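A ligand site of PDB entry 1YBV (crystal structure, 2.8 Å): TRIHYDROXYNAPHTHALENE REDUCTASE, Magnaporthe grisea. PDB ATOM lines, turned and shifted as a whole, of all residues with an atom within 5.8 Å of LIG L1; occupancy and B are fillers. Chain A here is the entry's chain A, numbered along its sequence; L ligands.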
ATOM      1  N   VAL A 118      -8.507  30.851  -2.974  1.00  0.00           N
ATOM      2  CA  VAL A 118      -9.223  30.214  -1.860  1.00  0.00           C
ATOM      3  C   VAL A 118      -8.293  29.911  -0.703  1.00  0.00           C
ATOM      4  O   VAL A 118      -7.080  29.950  -0.851  1.00  0.00           O
ATOM      5  CB  VAL A 118      -9.918  28.870  -2.214  1.00  0.00           C
ATOM      6  CG1 VAL A 118     -11.357  29.092  -2.589  1.00  0.00           C
ATOM      7  CG2 VAL A 118      -9.171  28.123  -3.291  1.00  0.00           C
ATOM      8  N   SER A 164     -18.986  35.302  -3.793  1.00  0.00           N
ATOM      9  CA  SER A 164     -19.129  33.861  -3.603  1.00  0.00           C
ATOM     10  C   SER A 164     -20.284  33.530  -2.678  1.00  0.00           C
ATOM     11  O   SER A 164     -20.696  34.341  -1.868  1.00  0.00           O
ATOM     12  CB  SER A 164     -17.851  33.275  -3.023  1.00  0.00           C
ATOM     13  OG  SER A 164     -18.039  31.916  -2.700  1.00  0.00           O
ATOM     14  N   ILE A 165     -20.766  32.296  -2.771  1.00  0.00           N
ATOM     15  CA  ILE A 165     -21.869  31.840  -1.931  1.00  0.00           C
ATOM     16  C   ILE A 165     -21.432  31.854  -0.455  1.00  0.00           C
ATOM     17  O   ILE A 165     -22.246  32.064   0.450  1.00  0.00           O
ATOM     18  CB  ILE A 165     -22.338  30.429  -2.327  1.00  0.00           C
ATOM     19  CG1 ILE A 165     -23.573  30.034  -1.524  1.00  0.00           C
ATOM     20  CG2 ILE A 165     -21.235  29.409  -2.107  1.00  0.00           C
ATOM     21  CD1 ILE A 165     -24.169  28.710  -1.914  1.00  0.00           C
ATOM     22  N   THR A 166     -20.127  31.703  -0.239  1.00  0.00           N
ATOM     23  CA  THR A 166     -19.544  31.692   1.094  1.00  0.00           C
ATOM     24  C   THR A 166     -19.673  33.033   1.802  1.00  0.00           C
ATOM     25  O   THR A 166     -19.430  33.117   2.998  1.00  0.00           O
ATOM     26  CB  THR A 166     -18.073  31.301   1.038  1.00  0.00           C
ATOM     27  OG1 THR A 166     -17.384  32.201   0.175  1.00  0.00           O
ATOM     28  CG2 THR A 166     -17.925  29.906   0.490  1.00  0.00           C
ATOM     29  N   HIS A 175     -13.445  28.246   7.206  1.00  0.00           N
ATOM     30  CA  HIS A 175     -13.512  29.063   6.009  1.00  0.00           C
ATOM     31  C   HIS A 175     -13.708  30.569   6.243  1.00  0.00           C
ATOM     32  O   HIS A 175     -14.113  31.281   5.325  1.00  0.00           O
ATOM     33  CB  HIS A 175     -14.638  28.508   5.129  1.00  0.00           C
ATOM     34  CG  HIS A 175     -14.341  28.539   3.671  1.00  0.00           C
ATOM     35  ND1 HIS A 175     -15.328  28.696   2.721  1.00  0.00           N
ATOM     36  CD2 HIS A 175     -13.177  28.411   3.000  1.00  0.00           C
ATOM     37  CE1 HIS A 175     -14.777  28.665   1.522  1.00  0.00           C
ATOM     38  NE2 HIS A 175     -13.478  28.489   1.659  1.00  0.00           N
ATOM     39  N   TYR A 178     -11.441  33.282   3.738  1.00  0.00           N
ATOM     40  CA  TYR A 178     -11.956  33.363   2.384  1.00  0.00           C
ATOM     41  C   TYR A 178     -13.378  33.941   2.384  1.00  0.00           C
ATOM     42  O   TYR A 178     -13.686  34.848   1.607  1.00  0.00           O
ATOM     43  CB  TYR A 178     -11.944  31.995   1.725  1.00  0.00           C
ATOM     44  CG  TYR A 178     -12.513  31.982   0.326  1.00  0.00           C
ATOM     45  CD1 TYR A 178     -11.814  32.542  -0.734  1.00  0.00           C
ATOM     46  CD2 TYR A 178     -13.750  31.405   0.074  1.00  0.00           C
ATOM     47  CE1 TYR A 178     -12.331  32.523  -2.019  1.00  0.00           C
ATOM     48  CE2 TYR A 178     -14.277  31.380  -1.198  1.00  0.00           C
ATOM     49  CZ  TYR A 178     -13.558  31.941  -2.244  1.00  0.00           C
ATOM     50  OH  TYR A 178     -14.094  31.911  -3.502  1.00  0.00           O
ATOM     51  N   PRO A 208     -21.312  33.227  -7.252  1.00  0.00           N
ATOM     52  CA  PRO A 208     -21.399  31.835  -7.687  1.00  0.00           C
ATOM     53  C   PRO A 208     -21.444  30.903  -6.493  1.00  0.00           C
ATOM     54  O   PRO A 208     -21.187  31.311  -5.368  1.00  0.00           O
ATOM     55  CB  PRO A 208     -20.094  31.657  -8.464  1.00  0.00           C
ATOM     56  CG  PRO A 208     -19.830  33.001  -8.992  1.00  0.00           C
ATOM     57  CD  PRO A 208     -20.111  33.861  -7.802  1.00  0.00           C
ATOM     58  N   GLY A 209     -21.694  29.626  -6.746  1.00  0.00           N
ATOM     59  CA  GLY A 209     -21.749  28.695  -5.646  1.00  0.00           C
ATOM     60  C   GLY A 209     -21.201  27.323  -5.955  1.00  0.00           C
ATOM     61  O   GLY A 209     -21.888  26.318  -5.704  1.00  0.00           O
ATOM     62  N   GLY A 210     -19.975  27.241  -6.448  1.00  0.00           N
ATOM     63  CA  GLY A 210     -19.424  25.913  -6.724  1.00  0.00           C
ATOM     64  C   GLY A 210     -19.487  25.624  -8.199  1.00  0.00           C
ATOM     65  O   GLY A 210     -20.468  25.044  -8.689  1.00  0.00           O
ATOM     66  N   ILE A 211     -18.422  25.996  -8.891  1.00  0.00           N
ATOM     67  CA  ILE A 211     -18.297  25.856 -10.327  1.00  0.00           C
ATOM     68  C   ILE A 211     -17.103  24.970 -10.661  1.00  0.00           C
ATOM     69  O   ILE A 211     -16.024  25.106 -10.056  1.00  0.00           O
ATOM     70  CB  ILE A 211     -18.082  27.243 -10.966  1.00  0.00           C
ATOM     71  CG1 ILE A 211     -19.171  28.224 -10.524  1.00  0.00           C
ATOM     72  CG2 ILE A 211     -17.992  27.129 -12.467  1.00  0.00           C
ATOM     73  CD1 ILE A 211     -20.578  27.863 -10.977  1.00  0.00           C
ATOM     74  N   MET A 215     -10.011  25.424  -9.453  1.00  0.00           N
ATOM     75  CA  MET A 215     -10.267  25.622  -8.019  1.00  0.00           C
ATOM     76  C   MET A 215     -11.136  24.490  -7.493  1.00  0.00           C
ATOM     77  O   MET A 215     -10.809  23.871  -6.475  1.00  0.00           O
ATOM     78  CB  MET A 215     -10.971  26.958  -7.764  1.00  0.00           C
ATOM     79  CG  MET A 215     -11.073  27.314  -6.287  1.00  0.00           C
ATOM     80  SD  MET A 215     -11.948  28.863  -5.942  1.00  0.00           S
ATOM     81  CE  MET A 215     -10.655  30.063  -6.298  1.00  0.00           C
ATOM     82  N   TYR A 216     -12.208  24.198  -8.205  1.00  0.00           N
ATOM     83  CA  TYR A 216     -13.130  23.138  -7.820  1.00  0.00           C
ATOM     84  C   TYR A 216     -12.371  21.825  -7.677  1.00  0.00           C
ATOM     85  O   TYR A 216     -12.545  21.111  -6.692  1.00  0.00           O
ATOM     86  CB  TYR A 216     -14.237  23.003  -8.870  1.00  0.00           C
ATOM     87  CG  TYR A 216     -15.242  21.896  -8.618  1.00  0.00           C
ATOM     88  CD1 TYR A 216     -15.033  20.616  -9.109  1.00  0.00           C
ATOM     89  CD2 TYR A 216     -16.442  22.176  -7.958  1.00  0.00           C
ATOM     90  CE1 TYR A 216     -16.016  19.619  -8.975  1.00  0.00           C
ATOM     91  CE2 TYR A 216     -17.417  21.191  -7.807  1.00  0.00           C
ATOM     92  CZ  TYR A 216     -17.199  19.916  -8.311  1.00  0.00           C
ATOM     93  OH  TYR A 216     -18.189  18.965  -8.217  1.00  0.00           O
ATOM     94  N   VAL A 219     -10.058  22.253  -4.312  1.00  0.00           N
ATOM     95  CA  VAL A 219     -10.650  22.285  -2.980  1.00  0.00           C
ATOM     96  C   VAL A 219     -12.093  21.880  -2.727  1.00  0.00           C
ATOM     97  O   VAL A 219     -12.578  22.057  -1.617  1.00  0.00           O
ATOM     98  CB  VAL A 219     -10.453  23.680  -2.395  1.00  0.00           C
ATOM     99  CG1 VAL A 219      -8.973  24.037  -2.384  1.00  0.00           C
ATOM    100  CG2 VAL A 219     -11.218  24.704  -3.219  1.00  0.00           C
ATOM    101  N   CYS A 220     -12.777  21.297  -3.705  1.00  0.00           N
ATOM    102  CA  CYS A 220     -14.162  20.909  -3.479  1.00  0.00           C
ATOM    103  C   CYS A 220     -14.356  20.016  -2.254  1.00  0.00           C
ATOM    104  O   CYS A 220     -15.263  20.240  -1.437  1.00  0.00           O
ATOM    105  CB  CYS A 220     -14.766  20.231  -4.718  1.00  0.00           C
ATOM    106  SG  CYS A 220     -16.535  19.833  -4.574  1.00  0.00           S
ATOM    107  N   TYR A 223     -15.302  21.123   1.203  1.00  0.00           N
ATOM    108  CA  TYR A 223     -16.668  21.548   1.484  1.00  0.00           C
ATOM    109  C   TYR A 223     -17.547  20.357   1.833  1.00  0.00           C
ATOM    110  O   TYR A 223     -18.615  20.523   2.423  1.00  0.00           O
ATOM    111  CB  TYR A 223     -17.272  22.246   0.262  1.00  0.00           C
ATOM    112  CG  TYR A 223     -16.686  23.590  -0.022  1.00  0.00           C
ATOM    113  CD1 TYR A 223     -15.589  23.731  -0.855  1.00  0.00           C
ATOM    114  CD2 TYR A 223     -17.247  24.740   0.530  1.00  0.00           C
ATOM    115  CE1 TYR A 223     -15.067  24.983  -1.138  1.00  0.00           C
ATOM    116  CE2 TYR A 223     -16.745  25.988   0.246  1.00  0.00           C
ATOM    117  CZ  TYR A 223     -15.654  26.105  -0.585  1.00  0.00           C
ATOM    118  OH  TYR A 223     -15.153  27.361  -0.874  1.00  0.00           O
ATOM    119  N   TRP A 243     -26.051  20.201  -3.363  1.00  0.00           N
ATOM    120  CA  TRP A 243     -26.111  21.643  -3.552  1.00  0.00           C
ATOM    121  C   TRP A 243     -27.098  22.258  -4.524  1.00  0.00           C
ATOM    122  O   TRP A 243     -27.055  23.461  -4.749  1.00  0.00           O
ATOM    123  CB  TRP A 243     -24.710  22.174  -3.859  1.00  0.00           C
ATOM    124  CG  TRP A 243     -23.757  21.915  -2.772  1.00  0.00           C
ATOM    125  CD1 TRP A 243     -24.026  21.900  -1.436  1.00  0.00           C
ATOM    126  CD2 TRP A 243     -22.359  21.652  -2.910  1.00  0.00           C
ATOM    127  NE1 TRP A 243     -22.879  21.650  -0.727  1.00  0.00           N
ATOM    128  CE2 TRP A 243     -21.840  21.490  -1.613  1.00  0.00           C
ATOM    129  CE3 TRP A 243     -21.500  21.537  -4.004  1.00  0.00           C
ATOM    130  CZ2 TRP A 243     -20.496  21.229  -1.376  1.00  0.00           C
ATOM    131  CZ3 TRP A 243     -20.155  21.276  -3.767  1.00  0.00           C
ATOM    132  CH2 TRP A 243     -19.669  21.123  -2.467  1.00  0.00           C
ATOM    133  N   MET A 283     -25.678  26.562   1.575  1.00  0.00           N
ATOM    134  CA  MET A 283     -24.414  26.228   2.229  1.00  0.00           C
ATOM    135  C   MET A 283     -24.198  26.971   3.551  1.00  0.00           C
ATOM    136  O   MET A 283     -23.108  26.820   4.126  1.00  0.00           O
ATOM    137  CB  MET A 283     -23.258  26.494   1.272  1.00  0.00           C
ATOM    138  CG  MET A 283     -23.299  25.619   0.033  1.00  0.00           C
ATOM    139  SD  MET A 283     -21.772  25.623  -0.918  1.00  0.00           S
ATOM    140  CE  MET A 283     -22.476  25.349  -2.576  1.00  0.00           C
ATOM    141  OXT MET A 283     -25.118  27.682   4.004  1.00  0.00           O
HETATM  142  C1  LIG L   1     -15.622  25.419  -4.650  1.00  0.00           C
HETATM  143  C2  LIG L   1     -14.234  25.744  -5.199  1.00  0.00           C
HETATM  144  C3  LIG L   1     -16.129  24.096  -4.707  1.00  0.00           C
HETATM  145  C4  LIG L   1     -17.403  23.760  -4.209  1.00  0.00           C
HETATM  146  C5  LIG L   1     -18.217  24.731  -3.628  1.00  0.00           C
HETATM  147  C6  LIG L   1     -17.720  26.051  -3.571  1.00  0.00           C
HETATM  148  C7  LIG L   1     -17.198  28.382  -3.306  1.00  0.00           C
HETATM  149  C8  LIG L   1     -16.466  26.384  -4.069  1.00  0.00           C
HETATM  150  C9  LIG L   1     -15.308  28.572  -4.071  1.00  0.00           C
HETATM  151  N1  LIG L   1     -16.264  27.708  -3.860  1.00  0.00           N
HETATM  152  N2  LIG L   1     -15.630  29.746  -3.705  1.00  0.00           N
HETATM  153  N3  LIG L   1     -16.938  29.604  -3.149  1.00  0.00           N
HETATM  154  S1  LIG L   1     -18.633  27.404  -2.873  1.00  0.00           S
HETATM  155  P1  LG2 L   2      -9.041  29.400 -10.647  1.00  0.00           P
HETATM  156  O1  LG2 L   2      -8.408  28.768  -9.461  1.00  0.00           O
HETATM  157  O2  LG2 L   2      -9.372  28.555 -11.830  1.00  0.00           O
HETATM  158  O3  LG2 L   2      -8.104  30.666 -11.045  1.00  0.00           O
HETATM  159  C1  LG2 L   2      -8.724  31.784 -11.734  1.00  0.00           C
HETATM  160  C2  LG2 L   2      -7.844  32.957 -11.957  1.00  0.00           C
HETATM  161  O4  LG2 L   2      -7.570  33.908 -10.934  1.00  0.00           O
HETATM  162  C3  LG2 L   2      -6.637  32.878 -12.836  1.00  0.00           C
HETATM  163  O5  LG2 L   2      -6.531  33.465 -13.976  1.00  0.00           O
HETATM  164  C4  LG2 L   2      -5.527  33.412 -11.947  1.00  0.00           C
HETATM  165  O6  LG2 L   2      -4.495  34.034 -12.763  1.00  0.00           O
HETATM  166  C5  LG2 L   2      -6.264  34.453 -11.131  1.00  0.00           C
HETATM  167  N1  LG2 L   2      -5.499  35.152 -10.258  1.00  0.00           N
HETATM  168  C6  LG2 L   2      -4.992  34.720  -9.096  1.00  0.00           C
HETATM  169  N2  LG2 L   2      -4.129  35.624  -8.621  1.00  0.00           N
HETATM  170  C7  LG2 L   2      -4.122  36.588  -9.513  1.00  0.00           C
HETATM  171  C8  LG2 L   2      -3.430  37.786  -9.422  1.00  0.00           C
HETATM  172  N3  LG2 L   2      -2.533  38.027  -8.468  1.00  0.00           N
HETATM  173  N4  LG2 L   2      -3.652  38.671 -10.421  1.00  0.00           N
HETATM  174  C9  LG2 L   2      -4.462  38.403 -11.443  1.00  0.00           C
HETATM  175  N5  LG2 L   2      -5.109  37.241 -11.526  1.00  0.00           N
HETATM  176  C10 LG2 L   2      -4.963  36.323 -10.563  1.00  0.00           C
HETATM  177  O7  LG2 L   2     -10.384  30.147 -10.167  1.00  0.00           O
HETATM  178  P2  LG2 L   2     -11.940  30.176 -10.595  1.00  0.00           P
HETATM  179  O8  LG2 L   2     -11.906  30.492 -12.049  1.00  0.00           O
HETATM  180  O9  LG2 L   2     -12.591  28.955 -10.065  1.00  0.00           O
HETATM  181  O10 LG2 L   2     -12.488  31.413  -9.721  1.00  0.00           O
HETATM  182  C11 LG2 L   2     -12.494  32.726 -10.282  1.00  0.00           C
HETATM  183  C12 LG2 L   2     -13.184  33.671  -9.325  1.00  0.00           C
HETATM  184  O11 LG2 L   2     -14.511  33.242  -8.988  1.00  0.00           O
HETATM  185  C13 LG2 L   2     -12.426  33.766  -8.023  1.00  0.00           C
HETATM  186  O12 LG2 L   2     -12.474  35.115  -7.542  1.00  0.00           O
HETATM  187  C14 LG2 L   2     -13.165  32.806  -7.108  1.00  0.00           C
HETATM  188  O13 LG2 L   2     -12.962  33.109  -5.730  1.00  0.00           O
HETATM  189  C15 LG2 L   2     -14.560  33.071  -7.561  1.00  0.00           C
HETATM  190  N6  LG2 L   2     -15.403  31.911  -7.249  1.00  0.00           N
HETATM  191  C16 LG2 L   2     -15.122  30.624  -7.752  1.00  0.00           C
HETATM  192  C17 LG2 L   2     -15.993  29.566  -7.478  1.00  0.00           C
HETATM  193  C18 LG2 L   2     -15.702  28.100  -7.830  1.00  0.00           C
HETATM  194  O14 LG2 L   2     -16.348  27.202  -7.312  1.00  0.00           O
HETATM  195  N7  LG2 L   2     -14.688  27.848  -8.666  1.00  0.00           N
HETATM  196  C19 LG2 L   2     -17.132  29.839  -6.726  1.00  0.00           C
HETATM  197  C20 LG2 L   2     -17.401  31.114  -6.227  1.00  0.00           C
HETATM  198  C21 LG2 L   2     -16.529  32.169  -6.487  1.00  0.00           C
HETATM  199  P3  LG2 L   2      -3.182  33.223 -13.221  1.00  0.00           P
HETATM  200  O15 LG2 L   2      -2.875  33.882 -14.496  1.00  0.00           O
HETATM  201  O16 LG2 L   2      -3.664  31.819 -13.344  1.00  0.00           O
HETATM  202  O17 LG2 L   2      -2.248  33.538 -12.096  1.00  0.00           O
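OG of Ser 164 lies within hydrogen-bond range of OG1 of Thr 166, at 3.0 Å. A ring nitrogen (NE2) of His 175 sits close to the side-chain hydroxyl (OH) of Tyr 223 (3.2 Å). N of Ile 165 is in hydrogen-bond range of O of Pro 208 (2.8 Å).
The side-chain hydroxyl (OG) of Ser 164 sits at hydrogen-bond distance from a nitrogen (N3) of LIG L1. The side-chain hydroxyl (OH) of Tyr 178 is in hydrogen-bond range of a nitrogen (N2) of LIG L1 (2.7 Å). The side-chain hydroxyl (OH) of Tyr 178 lies within hydrogen-bond range of an oxygen (O13) of LG2 L2 (2.8 Å). The backbone NH (N) of Ile 211 lies within hydrogen-bond range of an oxygen (O14) of LG2 L2. A nitrogen (N7) of LG2 L2 sits at hydrogen-bond distance from the backbone carbonyl oxygen of Ile 211 (3.4 Å).
OH of Tyr 223 lies close to N1 of LIG L1 (3.2 Å). Residues that only touch LIG L1: Ile 165 (3.4 Å), Thr 166 (3.8 Å), Gly 210 (3.5 Å), Met 215 (3.7 Å), Tyr 216 (3.8 Å), Val 219 (3.8 Å), Cys 220 (3.9 Å) and Trp 243 (3.7 Å). Hydrophobic or aromatic side chains within 4 Å of LIG L1: Ile 165, Tyr 178, Met 215, Tyr 216, Val 219, Tyr 223 and Trp 243. Of the 17 residues printed, 11 come within 4 Å of LIG L1.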
